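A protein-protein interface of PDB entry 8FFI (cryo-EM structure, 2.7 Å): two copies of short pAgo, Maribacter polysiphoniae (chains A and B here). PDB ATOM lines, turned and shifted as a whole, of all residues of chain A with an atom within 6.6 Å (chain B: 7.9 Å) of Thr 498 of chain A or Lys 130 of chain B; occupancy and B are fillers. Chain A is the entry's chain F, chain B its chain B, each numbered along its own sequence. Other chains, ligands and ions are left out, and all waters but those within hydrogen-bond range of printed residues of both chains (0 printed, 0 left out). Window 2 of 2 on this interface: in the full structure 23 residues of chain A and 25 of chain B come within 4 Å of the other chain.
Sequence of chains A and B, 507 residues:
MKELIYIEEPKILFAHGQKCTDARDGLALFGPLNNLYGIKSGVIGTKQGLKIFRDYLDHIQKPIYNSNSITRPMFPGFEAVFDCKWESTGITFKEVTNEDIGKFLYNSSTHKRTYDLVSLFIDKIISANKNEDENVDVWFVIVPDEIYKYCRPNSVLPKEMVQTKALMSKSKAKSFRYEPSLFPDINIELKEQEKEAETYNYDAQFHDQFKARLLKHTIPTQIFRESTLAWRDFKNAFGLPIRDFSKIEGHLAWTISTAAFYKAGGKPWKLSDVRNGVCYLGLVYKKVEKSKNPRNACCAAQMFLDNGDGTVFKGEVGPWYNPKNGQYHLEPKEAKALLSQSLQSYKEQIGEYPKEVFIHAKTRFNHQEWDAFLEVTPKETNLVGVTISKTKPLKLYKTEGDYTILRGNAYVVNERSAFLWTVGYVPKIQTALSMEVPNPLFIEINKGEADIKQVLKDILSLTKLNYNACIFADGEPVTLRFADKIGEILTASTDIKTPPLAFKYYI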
ATOM      1  N   LEU A 215     -15.316  21.518  16.166  1.00  0.00           N
ATOM      2  CA  LEU A 215     -15.067  20.221  15.546  1.00  0.00           C
ATOM      3  C   LEU A 215     -13.817  20.237  14.675  1.00  0.00           C
ATOM      4  O   LEU A 215     -13.115  19.226  14.578  1.00  0.00           O
ATOM      5  CB  LEU A 215     -16.278  19.798  14.716  1.00  0.00           C
ATOM      6  CG  LEU A 215     -17.244  18.792  15.342  1.00  0.00           C
ATOM      7  CD1 LEU A 215     -18.265  18.351  14.309  1.00  0.00           C
ATOM      8  CD2 LEU A 215     -16.493  17.599  15.911  1.00  0.00           C
ATOM      9  N   THR A 218     -10.835  19.970  17.170  1.00  0.00           N
ATOM     10  CA  THR A 218     -10.856  18.716  17.931  1.00  0.00           C
ATOM     11  C   THR A 218     -10.262  18.889  19.335  1.00  0.00           C
ATOM     12  O   THR A 218      -9.222  18.326  19.681  1.00  0.00           O
ATOM     13  CB  THR A 218     -10.133  17.595  17.171  1.00  0.00           C
ATOM     14  OG1 THR A 218      -8.727  17.870  17.119  1.00  0.00           O
ATOM     15  CG2 THR A 218     -10.671  17.471  15.757  1.00  0.00           C
ATOM     16  N   VAL A 317     -20.385   9.510   9.419  1.00  0.00           N
ATOM     17  CA  VAL A 317     -21.355  10.553   9.101  1.00  0.00           C
ATOM     18  C   VAL A 317     -20.725  11.594   8.182  1.00  0.00           C
ATOM     19  O   VAL A 317     -19.683  12.174   8.506  1.00  0.00           O
ATOM     20  CB  VAL A 317     -21.932  11.226  10.361  1.00  0.00           C
ATOM     21  CG1 VAL A 317     -22.680  10.214  11.202  1.00  0.00           C
ATOM     22  CG2 VAL A 317     -20.834  11.863  11.197  1.00  0.00           C
ATOM     23  N   ILE A 496     -19.221  23.256   8.328  1.00  0.00           N
ATOM     24  CA  ILE A 496     -18.440  22.075   8.674  1.00  0.00           C
ATOM     25  C   ILE A 496     -18.266  21.201   7.443  1.00  0.00           C
ATOM     26  O   ILE A 496     -19.229  20.927   6.715  1.00  0.00           O
ATOM     27  CB  ILE A 496     -19.109  21.285   9.814  1.00  0.00           C
ATOM     28  CG1 ILE A 496     -19.585  22.232  10.915  1.00  0.00           C
ATOM     29  CG2 ILE A 496     -18.146  20.254  10.380  1.00  0.00           C
ATOM     30  CD1 ILE A 496     -20.302  21.534  12.048  1.00  0.00           C
ATOM     31  N   LYS A 497     -17.032  20.763   7.207  1.00  0.00           N
ATOM     32  CA  LYS A 497     -16.721  19.788   6.175  1.00  0.00           C
ATOM     33  C   LYS A 497     -15.872  18.682   6.785  1.00  0.00           C
ATOM     34  O   LYS A 497     -15.095  18.920   7.714  1.00  0.00           O
ATOM     35  CB  LYS A 497     -15.987  20.425   4.984  1.00  0.00           C
ATOM     36  CG  LYS A 497     -14.605  20.964   5.311  1.00  0.00           C
ATOM     37  CD  LYS A 497     -13.905  21.486   4.067  1.00  0.00           C
ATOM     38  CE  LYS A 497     -12.506  21.986   4.390  1.00  0.00           C
ATOM     39  NZ  LYS A 497     -11.631  20.889   4.890  1.00  0.00           N
ATOM     40  N   THR A 498     -16.035  17.464   6.245  1.00  0.00           N
ATOM     41  CA  THR A 498     -15.404  16.219   6.686  1.00  0.00           C
ATOM     42  C   THR A 498     -15.214  16.166   8.203  1.00  0.00           C
ATOM     43  O   THR A 498     -14.078  16.115   8.691  1.00  0.00           O
ATOM     44  CB  THR A 498     -14.073  15.983   5.948  1.00  0.00           C
ATOM     45  OG1 THR A 498     -13.459  14.779   6.426  1.00  0.00           O
ATOM     46  CG2 THR A 498     -13.094  17.161   6.069  1.00  0.00           C
ATOM     47  N   PRO A 499     -16.297  16.154   8.978  1.00  0.00           N
ATOM     48  CA  PRO A 499     -16.170  16.156  10.442  1.00  0.00           C
ATOM     49  C   PRO A 499     -15.570  14.853  10.938  1.00  0.00           C
ATOM     50  O   PRO A 499     -15.631  13.827  10.243  1.00  0.00           O
ATOM     51  CB  PRO A 499     -17.620  16.326  10.929  1.00  0.00           C
ATOM     52  CG  PRO A 499     -18.440  16.615   9.708  1.00  0.00           C
ATOM     53  CD  PRO A 499     -17.699  16.044   8.550  1.00  0.00           C
ATOM     54  N   PRO A 500     -14.980  14.850  12.133  1.00  0.00           N
ATOM     55  CA  PRO A 500     -14.349  13.628  12.646  1.00  0.00           C
ATOM     56  C   PRO A 500     -15.380  12.553  12.950  1.00  0.00           C
ATOM     57  O   PRO A 500     -16.594  12.760  12.868  1.00  0.00           O
ATOM     58  CB  PRO A 500     -13.637  14.095  13.921  1.00  0.00           C
ATOM     59  CG  PRO A 500     -13.623  15.597  13.849  1.00  0.00           C
ATOM     60  CD  PRO A 500     -14.833  15.977  13.066  1.00  0.00           C
ATOM     61  N   LEU A 501     -14.875  11.379  13.322  1.00  0.00           N
ATOM     62  CA  LEU A 501     -15.728  10.239  13.626  1.00  0.00           C
ATOM     63  C   LEU A 501     -15.729   9.847  15.094  1.00  0.00           C
ATOM     64  O   LEU A 501     -16.690   9.228  15.551  1.00  0.00           O
ATOM     65  CB  LEU A 501     -15.314   9.021  12.790  1.00  0.00           C
ATOM     66  CG  LEU A 501     -15.313   9.196  11.270  1.00  0.00           C
ATOM     67  CD1 LEU A 501     -15.172   7.850  10.573  1.00  0.00           C
ATOM     68  CD2 LEU A 501     -16.563   9.922  10.802  1.00  0.00           C
ATOM     69  N   ALA A 502     -14.679  10.187  15.839  1.00  0.00           N
ATOM     70  CA  ALA A 502     -14.610   9.825  17.248  1.00  0.00           C
ATOM     71  C   ALA A 502     -15.728  10.501  18.033  1.00  0.00           C
ATOM     72  O   ALA A 502     -16.086  11.652  17.773  1.00  0.00           O
ATOM     73  CB  ALA A 502     -13.248  10.209  17.826  1.00  0.00           C
ATOM     74  N   TYR A 505     -15.580  14.026  20.740  1.00  0.00           N
ATOM     75  CA  TYR A 505     -15.803  15.424  20.406  1.00  0.00           C
ATOM     76  C   TYR A 505     -17.278  15.775  20.263  1.00  0.00           C
ATOM     77  O   TYR A 505     -17.598  16.929  19.963  1.00  0.00           O
ATOM     78  CB  TYR A 505     -15.051  15.781  19.121  1.00  0.00           C
ATOM     79  CG  TYR A 505     -13.623  15.291  19.109  1.00  0.00           C
ATOM     80  CD1 TYR A 505     -12.700  15.753  20.040  1.00  0.00           C
ATOM     81  CD2 TYR A 505     -13.194  14.366  18.170  1.00  0.00           C
ATOM     82  CE1 TYR A 505     -11.393  15.306  20.033  1.00  0.00           C
ATOM     83  CE2 TYR A 505     -11.890  13.912  18.156  1.00  0.00           C
ATOM     84  CZ  TYR A 505     -10.994  14.385  19.089  1.00  0.00           C
ATOM     85  OH  TYR A 505      -9.694  13.937  19.077  1.00  0.00           O
ATOM     86  N   ASP B 123      -1.382  11.539   5.764  1.00  0.00           N
ATOM     87  CA  ASP B 123      -2.732  10.998   5.644  1.00  0.00           C
ATOM     88  C   ASP B 123      -3.033  10.038   6.786  1.00  0.00           C
ATOM     89  O   ASP B 123      -4.075  10.144   7.443  1.00  0.00           O
ATOM     90  CB  ASP B 123      -2.903  10.305   4.293  1.00  0.00           C
ATOM     91  CG  ASP B 123      -3.181  11.283   3.165  1.00  0.00           C
ATOM     92  OD1 ASP B 123      -3.903  12.275   3.402  1.00  0.00           O
ATOM     93  OD2 ASP B 123      -2.683  11.057   2.043  1.00  0.00           O
ATOM     94  N   LYS B 124      -2.119   9.100   7.047  1.00  0.00           N
ATOM     95  CA  LYS B 124      -2.311   8.176   8.159  1.00  0.00           C
ATOM     96  C   LYS B 124      -2.316   8.906   9.495  1.00  0.00           C
ATOM     97  O   LYS B 124      -3.144   8.609  10.365  1.00  0.00           O
ATOM     98  CB  LYS B 124      -1.233   7.095   8.146  1.00  0.00           C
ATOM     99  CG  LYS B 124      -1.518   5.954   7.197  1.00  0.00           C
ATOM    100  CD  LYS B 124      -0.298   5.074   7.004  1.00  0.00           C
ATOM    101  CE  LYS B 124      -0.579   3.979   5.992  1.00  0.00           C
ATOM    102  NZ  LYS B 124      -0.897   4.536   4.651  1.00  0.00           N
ATOM    103  N   ILE B 125      -1.408   9.870   9.679  1.00  0.00           N
ATOM    104  CA  ILE B 125      -1.368  10.586  10.956  1.00  0.00           C
ATOM    105  C   ILE B 125      -2.679  11.335  11.195  1.00  0.00           C
ATOM    106  O   ILE B 125      -3.271  11.265  12.282  1.00  0.00           O
ATOM    107  CB  ILE B 125      -0.155  11.532  11.010  1.00  0.00           C
ATOM    108  CG1 ILE B 125       1.145  10.728  10.969  1.00  0.00           C
ATOM    109  CG2 ILE B 125      -0.196  12.375  12.270  1.00  0.00           C
ATOM    110  CD1 ILE B 125       2.388  11.579  11.021  1.00  0.00           C
ATOM    111  N   ILE B 126      -3.163  12.048  10.173  1.00  0.00           N
ATOM    112  CA  ILE B 126      -4.387  12.832  10.297  1.00  0.00           C
ATOM    113  C   ILE B 126      -5.588  11.923  10.524  1.00  0.00           C
ATOM    114  O   ILE B 126      -6.451  12.213  11.364  1.00  0.00           O
ATOM    115  CB  ILE B 126      -4.570  13.715   9.049  1.00  0.00           C
ATOM    116  CG1 ILE B 126      -3.603  14.897   9.085  1.00  0.00           C
ATOM    117  CG2 ILE B 126      -6.002  14.202   8.936  1.00  0.00           C
ATOM    118  CD1 ILE B 126      -3.316  15.489   7.721  1.00  0.00           C
ATOM    119  N   SER B 127      -5.674  10.819   9.778  1.00  0.00           N
ATOM    120  CA  SER B 127      -6.793   9.900   9.951  1.00  0.00           C
ATOM    121  C   SER B 127      -6.809   9.310  11.353  1.00  0.00           C
ATOM    122  O   SER B 127      -7.873   9.199  11.974  1.00  0.00           O
ATOM    123  CB  SER B 127      -6.728   8.789   8.903  1.00  0.00           C
ATOM    124  OG  SER B 127      -5.947   7.702   9.365  1.00  0.00           O
ATOM    125  N   ALA B 128      -5.639   8.925  11.872  1.00  0.00           N
ATOM    126  CA  ALA B 128      -5.575   8.405  13.233  1.00  0.00           C
ATOM    127  C   ALA B 128      -6.009   9.456  14.247  1.00  0.00           C
ATOM    128  O   ALA B 128      -6.724   9.144  15.205  1.00  0.00           O
ATOM    129  CB  ALA B 128      -4.166   7.907  13.541  1.00  0.00           C
ATOM    130  N   ASN B 129      -5.583  10.708  14.058  1.00  0.00           N
ATOM    131  CA  ASN B 129      -5.980  11.759  14.991  1.00  0.00           C
ATOM    132  C   ASN B 129      -7.488  11.993  14.963  1.00  0.00           C
ATOM    133  O   ASN B 129      -8.122  12.129  16.015  1.00  0.00           O
ATOM    134  CB  ASN B 129      -5.234  13.056  14.670  1.00  0.00           C
ATOM    135  CG  ASN B 129      -5.440  14.133  15.727  1.00  0.00           C
ATOM    136  OD1 ASN B 129      -4.891  15.230  15.636  1.00  0.00           O
ATOM    137  ND2 ASN B 129      -6.227  13.813  16.744  1.00  0.00           N
ATOM    138  N   LYS B 130      -8.081  12.036  13.768  1.00  0.00           N
ATOM    139  CA  LYS B 130      -9.473  12.467  13.647  1.00  0.00           C
ATOM    140  C   LYS B 130     -10.447  11.412  14.159  1.00  0.00           C
ATOM    141  O   LYS B 130     -11.405  11.740  14.868  1.00  0.00           O
ATOM    142  CB  LYS B 130      -9.789  12.814  12.193  1.00  0.00           C
ATOM    143  CG  LYS B 130      -9.343  14.197  11.766  1.00  0.00           C
ATOM    144  CD  LYS B 130      -9.839  14.524  10.368  1.00  0.00           C
ATOM    145  CE  LYS B 130     -11.339  14.741  10.356  1.00  0.00           C
ATOM    146  NZ  LYS B 130     -11.748  15.665   9.265  1.00  0.00           N
ATOM    147  N   ASN B 131     -10.226  10.145  13.812  1.00  0.00           N
ATOM    148  CA  ASN B 131     -11.254   9.124  13.980  1.00  0.00           C
ATOM    149  C   ASN B 131     -10.781   7.938  14.810  1.00  0.00           C
ATOM    150  O   ASN B 131     -10.943   6.790  14.387  1.00  0.00           O
ATOM    151  CB  ASN B 131     -11.730   8.618  12.616  1.00  0.00           C
ATOM    152  CG  ASN B 131     -11.920   9.731  11.607  1.00  0.00           C
ATOM    153  OD1 ASN B 131     -12.341  10.834  11.949  1.00  0.00           O
ATOM    154  ND2 ASN B 131     -11.612   9.443  10.349  1.00  0.00           N
ATOM    155  N   GLU B 132     -10.189   8.188  15.974  1.00  0.00           N
ATOM    156  CA  GLU B 132      -9.760   7.099  16.842  1.00  0.00           C
ATOM    157  C   GLU B 132      -9.916   7.516  18.296  1.00  0.00           C
ATOM    158  O   GLU B 132     -10.157   8.685  18.610  1.00  0.00           O
ATOM    159  CB  GLU B 132      -8.318   6.675  16.546  1.00  0.00           C
ATOM    160  CG  GLU B 132      -8.199   5.610  15.476  1.00  0.00           C
ATOM    161  CD  GLU B 132      -6.858   4.913  15.495  1.00  0.00           C
ATOM    162  OE1 GLU B 132      -5.945   5.399  16.193  1.00  0.00           O
ATOM    163  OE2 GLU B 132      -6.717   3.876  14.815  1.00  0.00           O
ATOM    164  N   ASP B 133      -9.773   6.535  19.186  1.00  0.00           N
ATOM    165  CA  ASP B 133      -9.995   6.716  20.616  1.00  0.00           C
ATOM    166  C   ASP B 133      -8.706   6.879  21.411  1.00  0.00           C
ATOM    167  O   ASP B 133      -8.695   7.593  22.418  1.00  0.00           O
ATOM    168  CB  ASP B 133     -10.786   5.532  21.181  1.00  0.00           C
ATOM    169  CG  ASP B 133     -12.281   5.688  20.989  1.00  0.00           C
ATOM    170  OD1 ASP B 133     -12.868   6.591  21.621  1.00  0.00           O
ATOM    171  OD2 ASP B 133     -12.868   4.909  20.209  1.00  0.00           O
ATOM    172  N   HIS B 217      -3.264  21.160  11.939  1.00  0.00           N
ATOM    173  CA  HIS B 217      -3.822  20.142  12.814  1.00  0.00           C
ATOM    174  C   HIS B 217      -3.215  20.158  14.211  1.00  0.00           C
ATOM    175  O   HIS B 217      -3.820  19.604  15.135  1.00  0.00           O
ATOM    176  CB  HIS B 217      -3.638  18.754  12.192  1.00  0.00           C
ATOM    177  CG  HIS B 217      -4.294  18.601  10.856  1.00  0.00           C
ATOM    178  ND1 HIS B 217      -5.650  18.764  10.669  1.00  0.00           N
ATOM    179  CD2 HIS B 217      -3.779  18.315   9.637  1.00  0.00           C
ATOM    180  CE1 HIS B 217      -5.943  18.575   9.395  1.00  0.00           C
ATOM    181  NE2 HIS B 217      -4.825  18.303   8.747  1.00  0.00           N
ATOM    182  N   ILE B 219      -0.274  18.789  15.661  1.00  0.00           N
ATOM    183  CA  ILE B 219       0.149  17.484  16.161  1.00  0.00           C
ATOM    184  C   ILE B 219       1.647  17.521  16.436  1.00  0.00           C
ATOM    185  O   ILE B 219       2.445  17.611  15.492  1.00  0.00           O
ATOM    186  CB  ILE B 219      -0.190  16.365  15.163  1.00  0.00           C
ATOM    187  CG1 ILE B 219      -1.702  16.183  15.051  1.00  0.00           C
ATOM    188  CG2 ILE B 219       0.477  15.063  15.570  1.00  0.00           C
ATOM    189  CD1 ILE B 219      -2.164  15.875  13.652  1.00  0.00           C
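Of the 11 printed residues of chain A, 5 touch a printed residue of chain B.
Hydrophobic or aromatic side chains of chain A within 4 Å of the printed part of chain B: Pro 500, Leu 501, Ala 502 and Tyr 505.
Of the 13 printed residues of chain B, 4 touch a printed residue of chain A.
Among the printed residues, 9 pairs touch across the chains.
Among the printed residues, no Asp or Glu carboxylate lies within 4 Å of a Lys or Arg side-chain nitrogen of the other chain.
No position is printed for both chains.
Lys 130 of chain B touches Pro 500 of chain A.
OD1 of Asn 131 of chain B touches CA of Pro 500 of chain A, at 3.5 Å.
Leu 501 of chain A touches Lys 130 of chain B.
Lys 130 of chain B touches Ala 502 of chain A (O to N, 3.8 Å).
Glu 132 of chain B touches Ala 502 of chain A (O to CB, 3.5 Å).
OH of Tyr 505 of chain A touches O of Asn 129 of chain B (3.9 Å).
Tyr 505 of chain A touches Lys 130 of chain B (CE2 to O, 3.97 Å).
O of Thr 498 of chain A lies within hydrogen-bond range of NZ of Lys 130 of chain B (2.4 Å).
The side-chain amide oxygen (OD1) of Asn 131 of chain B is in hydrogen-bond range of the backbone NH (N) of Leu 501 of chain A, 2.9 Å away.
Of chain B, only Lys 130 (2.4 Å) comes within 4 Å of Thr 498 of chain A.
No residue of chain B comes within 4 Å of Pro 499 of chain A.
Of the printed residues of chain B, Pro 500 of chain A touches Lys 130 and Asn 131.
Of the printed residues of chain B, Leu 501 of chain A touches Lys 130 (3.8 Å) and Asn 131 (2.9 Å).
Printed residues of chain B within 4 Å of Ala 502 of chain A: Lys 130 and Glu 132.
Printed residues of chain A within 4 Å of Asn 129 of chain B: Tyr 505.
Printed residues of chain A within 4 Å of Glu 132 of chain B: Ala 502.
The nearest residue of chain B that does not touch Thr 498 of chain A is Asn 131 of chain B (6.4 Å).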
